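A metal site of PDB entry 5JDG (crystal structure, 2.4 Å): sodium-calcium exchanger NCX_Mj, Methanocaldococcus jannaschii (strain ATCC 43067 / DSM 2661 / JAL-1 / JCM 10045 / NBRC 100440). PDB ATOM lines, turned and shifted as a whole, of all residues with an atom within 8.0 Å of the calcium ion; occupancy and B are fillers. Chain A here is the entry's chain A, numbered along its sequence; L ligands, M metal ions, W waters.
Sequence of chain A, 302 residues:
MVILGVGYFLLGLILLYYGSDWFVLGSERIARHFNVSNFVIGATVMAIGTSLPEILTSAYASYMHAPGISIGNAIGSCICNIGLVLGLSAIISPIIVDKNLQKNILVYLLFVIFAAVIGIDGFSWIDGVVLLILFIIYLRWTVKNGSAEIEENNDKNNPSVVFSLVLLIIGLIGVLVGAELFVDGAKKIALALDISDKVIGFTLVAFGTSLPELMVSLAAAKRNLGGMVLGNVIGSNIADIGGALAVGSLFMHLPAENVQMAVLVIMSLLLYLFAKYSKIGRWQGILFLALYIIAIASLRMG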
ATOM      1  N   ALA A 115      14.694 -12.884  -5.335  1.00  0.00           N
ATOM      2  CA  ALA A 115      14.700 -13.802  -6.466  1.00  0.00           C
ATOM      3  C   ALA A 115      16.081 -14.408  -6.686  1.00  0.00           C
ATOM      4  O   ALA A 115      16.206 -15.602  -6.972  1.00  0.00           O
ATOM      5  CB  ALA A 115      14.229 -13.097  -7.731  1.00  0.00           C
ATOM      6  N   ALA A 116      17.114 -13.590  -6.534  1.00  0.00           N
ATOM      7  CA  ALA A 116      18.487 -14.038  -6.723  1.00  0.00           C
ATOM      8  C   ALA A 116      18.889 -15.060  -5.665  1.00  0.00           C
ATOM      9  O   ALA A 116      19.564 -16.041  -5.964  1.00  0.00           O
ATOM     10  CB  ALA A 116      19.445 -12.858  -6.689  1.00  0.00           C
ATOM     11  N   VAL A 117      18.445 -14.838  -4.433  1.00  0.00           N
ATOM     12  CA  VAL A 117      18.780 -15.738  -3.328  1.00  0.00           C
ATOM     13  C   VAL A 117      18.108 -17.096  -3.482  1.00  0.00           C
ATOM     14  O   VAL A 117      18.749 -18.136  -3.328  1.00  0.00           O
ATOM     15  CB  VAL A 117      18.404 -15.116  -1.971  1.00  0.00           C
ATOM     16  CG1 VAL A 117      18.514 -16.153  -0.868  1.00  0.00           C
ATOM     17  CG2 VAL A 117      19.285 -13.915  -1.666  1.00  0.00           C
ATOM     18  N   ILE A 118      16.808 -17.096  -3.786  1.00  0.00           N
ATOM     19  CA  ILE A 118      16.079 -18.347  -3.949  1.00  0.00           C
ATOM     20  C   ILE A 118      16.409 -19.027  -5.275  1.00  0.00           C
ATOM     21  O   ILE A 118      16.052 -20.184  -5.487  1.00  0.00           O
ATOM     22  CB  ILE A 118      14.542 -18.135  -3.863  1.00  0.00           C
ATOM     23  CG1 ILE A 118      14.031 -17.403  -5.097  1.00  0.00           C
ATOM     24  CG2 ILE A 118      14.174 -17.398  -2.580  1.00  0.00           C
ATOM     25  CD1 ILE A 118      12.525 -17.238  -5.134  1.00  0.00           C
ATOM     26  N   GLY A 119      17.100 -18.317  -6.148  1.00  0.00           N
ATOM     27  CA  GLY A 119      17.478 -18.871  -7.444  1.00  0.00           C
ATOM     28  C   GLY A 119      18.877 -19.464  -7.451  1.00  0.00           C
ATOM     29  O   GLY A 119      19.308 -20.005  -8.470  1.00  0.00           O
ATOM     30  N   ILE A 120      19.571 -19.360  -6.317  1.00  0.00           N
ATOM     31  CA  ILE A 120      20.920 -19.884  -6.181  1.00  0.00           C
ATOM     32  C   ILE A 120      21.000 -21.369  -6.551  1.00  0.00           C
ATOM     33  O   ILE A 120      21.926 -21.798  -7.226  1.00  0.00           O
ATOM     34  CB  ILE A 120      21.451 -19.689  -4.740  1.00  0.00           C
ATOM     35  CG1 ILE A 120      21.702 -18.199  -4.470  1.00  0.00           C
ATOM     36  CG2 ILE A 120      22.735 -20.477  -4.521  1.00  0.00           C
ATOM     37  CD1 ILE A 120      22.166 -17.915  -3.056  1.00  0.00           C
ATOM     38  N   ASP A 121      20.004 -22.134  -6.101  1.00  0.00           N
ATOM     39  CA  ASP A 121      19.918 -23.544  -6.438  1.00  0.00           C
ATOM     40  C   ASP A 121      18.932 -23.776  -7.578  1.00  0.00           C
ATOM     41  O   ASP A 121      18.383 -24.872  -7.717  1.00  0.00           O
ATOM     42  CB  ASP A 121      19.518 -24.362  -5.210  1.00  0.00           C
ATOM     43  CG  ASP A 121      18.198 -23.904  -4.613  1.00  0.00           C
ATOM     44  OD1 ASP A 121      17.723 -22.816  -4.995  1.00  0.00           O
ATOM     45  OD2 ASP A 121      17.640 -24.634  -3.764  1.00  0.00           O
ATOM     46  N   GLY A 122      18.714 -22.742  -8.378  1.00  0.00           N
ATOM     47  CA  GLY A 122      17.763 -22.822  -9.474  1.00  0.00           C
ATOM     48  C   GLY A 122      16.370 -22.386  -9.047  1.00  0.00           C
ATOM     49  O   GLY A 122      16.130 -22.144  -7.870  1.00  0.00           O
ATOM     50  N   PHE A 123      15.444 -22.297 -10.001  1.00  0.00           N
ATOM     51  CA  PHE A 123      14.082 -21.909  -9.696  1.00  0.00           C
ATOM     52  C   PHE A 123      13.107 -23.070  -9.855  1.00  0.00           C
ATOM     53  O   PHE A 123      12.907 -23.585 -10.951  1.00  0.00           O
ATOM     54  CB  PHE A 123      13.631 -20.748 -10.594  1.00  0.00           C
ATOM     55  CG  PHE A 123      14.343 -19.448 -10.309  1.00  0.00           C
ATOM     56  CD1 PHE A 123      13.939 -18.633  -9.275  1.00  0.00           C
ATOM     57  CD2 PHE A 123      15.425 -19.059 -11.074  1.00  0.00           C
ATOM     58  CE1 PHE A 123      14.585 -17.444  -9.015  1.00  0.00           C
ATOM     59  CE2 PHE A 123      16.086 -17.873 -10.830  1.00  0.00           C
ATOM     60  CZ  PHE A 123      15.669 -17.062  -9.796  1.00  0.00           C
ATOM     61  N   SER A 124      12.510 -23.487  -8.746  1.00  0.00           N
ATOM     62  CA  SER A 124      11.491 -24.535  -8.766  1.00  0.00           C
ATOM     63  C   SER A 124      10.120 -23.935  -9.007  1.00  0.00           C
ATOM     64  O   SER A 124       9.942 -22.716  -8.983  1.00  0.00           O
ATOM     65  CB  SER A 124      11.501 -25.317  -7.458  1.00  0.00           C
ATOM     66  OG  SER A 124      10.961 -24.545  -6.400  1.00  0.00           O
ATOM     67  N   TRP A 125       9.132 -24.798  -9.238  1.00  0.00           N
ATOM     68  CA  TRP A 125       7.777 -24.354  -9.517  1.00  0.00           C
ATOM     69  C   TRP A 125       7.182 -23.632  -8.302  1.00  0.00           C
ATOM     70  O   TRP A 125       6.316 -22.773  -8.448  1.00  0.00           O
ATOM     71  CB  TRP A 125       6.892 -25.531  -9.918  1.00  0.00           C
ATOM     72  CG  TRP A 125       6.801 -26.609  -8.883  1.00  0.00           C
ATOM     73  CD1 TRP A 125       7.632 -27.667  -8.726  1.00  0.00           C
ATOM     74  CD2 TRP A 125       5.803 -26.724  -7.857  1.00  0.00           C
ATOM     75  NE1 TRP A 125       7.230 -28.432  -7.667  1.00  0.00           N
ATOM     76  CE2 TRP A 125       6.108 -27.873  -7.111  1.00  0.00           C
ATOM     77  CE3 TRP A 125       4.685 -25.956  -7.498  1.00  0.00           C
ATOM     78  CZ2 TRP A 125       5.330 -28.285  -6.029  1.00  0.00           C
ATOM     79  CZ3 TRP A 125       3.921 -26.366  -6.416  1.00  0.00           C
ATOM     80  CH2 TRP A 125       4.250 -27.526  -5.696  1.00  0.00           C
ATOM     81  N   ILE A 126       7.666 -23.988  -7.119  1.00  0.00           N
ATOM     82  CA  ILE A 126       7.258 -23.306  -5.899  1.00  0.00           C
ATOM     83  C   ILE A 126       7.871 -21.897  -5.868  1.00  0.00           C
ATOM     84  O   ILE A 126       7.221 -20.941  -5.452  1.00  0.00           O
ATOM     85  CB  ILE A 126       7.671 -24.085  -4.636  1.00  0.00           C
ATOM     86  CG1 ILE A 126       7.010 -25.470  -4.630  1.00  0.00           C
ATOM     87  CG2 ILE A 126       7.290 -23.322  -3.382  1.00  0.00           C
ATOM     88  CD1 ILE A 126       7.261 -26.268  -3.372  1.00  0.00           C
ATOM     89  N   ASP A 127       9.120 -21.792  -6.301  1.00  0.00           N
ATOM     90  CA  ASP A 127       9.768 -20.490  -6.443  1.00  0.00           C
ATOM     91  C   ASP A 127       8.960 -19.605  -7.387  1.00  0.00           C
ATOM     92  O   ASP A 127       8.807 -18.412  -7.160  1.00  0.00           O
ATOM     93  CB  ASP A 127      11.201 -20.631  -6.967  1.00  0.00           C
ATOM     94  CG  ASP A 127      12.139 -21.212  -5.924  1.00  0.00           C
ATOM     95  OD1 ASP A 127      11.905 -20.999  -4.710  1.00  0.00           O
ATOM     96  OD2 ASP A 127      13.128 -21.869  -6.316  1.00  0.00           O
ATOM     97  N   GLY A 128       8.439 -20.208  -8.455  1.00  0.00           N
ATOM     98  CA  GLY A 128       7.627 -19.497  -9.420  1.00  0.00           C
ATOM     99  C   GLY A 128       6.333 -18.986  -8.804  1.00  0.00           C
ATOM    100  O   GLY A 128       5.953 -17.838  -9.022  1.00  0.00           O
ATOM    101  N   HIS A 253      12.047 -27.117 -13.829  1.00  0.00           N
ATOM    102  CA  HIS A 253      13.051 -26.476 -13.005  1.00  0.00           C
ATOM    103  C   HIS A 253      14.044 -25.683 -13.855  1.00  0.00           C
ATOM    104  O   HIS A 253      14.624 -26.215 -14.797  1.00  0.00           O
ATOM    105  CB  HIS A 253      13.802 -27.511 -12.168  1.00  0.00           C
ATOM    106  CG  HIS A 253      14.716 -26.930 -11.136  1.00  0.00           C
ATOM    107  ND1 HIS A 253      14.271 -26.512  -9.893  1.00  0.00           N
ATOM    108  CD2 HIS A 253      16.049 -26.673 -11.156  1.00  0.00           C
ATOM    109  CE1 HIS A 253      15.293 -26.035  -9.197  1.00  0.00           C
ATOM    110  NE2 HIS A 253      16.380 -26.130  -9.950  1.00  0.00           N
ATOM    111  N   LEU A 254      14.205 -24.403 -13.531  1.00  0.00           N
ATOM    112  CA  LEU A 254      15.142 -23.550 -14.248  1.00  0.00           C
ATOM    113  C   LEU A 254      16.509 -23.608 -13.582  1.00  0.00           C
ATOM    114  O   LEU A 254      16.623 -23.367 -12.383  1.00  0.00           O
ATOM    115  CB  LEU A 254      14.627 -22.110 -14.309  1.00  0.00           C
ATOM    116  CG  LEU A 254      13.177 -21.920 -14.735  1.00  0.00           C
ATOM    117  CD1 LEU A 254      12.812 -20.439 -14.763  1.00  0.00           C
ATOM    118  CD2 LEU A 254      12.915 -22.557 -16.092  1.00  0.00           C
ATOM    119  N   ALA A 256      20.288 -22.583 -12.368  1.00  0.00           N
ATOM    120  CA  ALA A 256      20.718 -21.327 -11.748  1.00  0.00           C
ATOM    121  C   ALA A 256      21.525 -20.459 -12.703  1.00  0.00           C
ATOM    122  O   ALA A 256      22.443 -20.923 -13.373  1.00  0.00           O
ATOM    123  CB  ALA A 256      21.529 -21.618 -10.497  1.00  0.00           C
HETATM  124  C1  LIG L   1      14.222 -21.830  -2.648  1.00  0.00           C
HETATM  125  C2  LIG L   1      19.758 -21.159  -0.019  1.00  0.00           C
HETATM  126  C3  LIG L   1      16.591 -21.632  -1.872  1.00  0.00           C
HETATM  127  C4  LIG L   1      18.745 -21.399  -1.145  1.00  0.00           C
HETATM  128  C5  LIG L   1      15.124 -21.570  -1.433  1.00  0.00           C
HETATM  129  O1  LIG L   1      19.118 -21.590  -2.301  1.00  0.00           O
HETATM  130  O2  LIG L   1      14.511 -23.119  -3.182  1.00  0.00           O
HETATM  131  O3  LIG L   1      14.882 -22.572  -0.438  1.00  0.00           O
HETATM  132  O4  LIG L   1      17.437 -21.382  -0.744  1.00  0.00           O
HETATM  133 CA    CA M   1      15.387 -22.428  -5.657  1.00  0.00          CA
HETATM  134  O   HOH W   1      14.315 -24.680  -5.892  1.00  0.00           O
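The side-chain hydroxyl of Ser 124 lies within hydrogen-bond range of the backbone NH of Asp 127, at 3.3 Å.
O of Asp 121 is in hydrogen-bond range of NE2 of His 253 (3.3 Å).
Within 4 Å of the calcium ion: Ile 118, Asp 121, Gly 122 and Asp 127.
O of Ile 118 is bound to the calcium ion (2.3 Å).
O of Gly 122 binds the calcium ion (2.4 Å).
OD2 of Asp 127 binds the calcium ion (2.4 Å).
OD1 of Asp 121 binds the calcium ion.
Water W1 is bound to the calcium ion, 2.5 Å away.
An oxygen (O2) of the ligand is bound to the calcium ion (2.7 Å).
The calcium ion has six donor atoms within binding distance.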
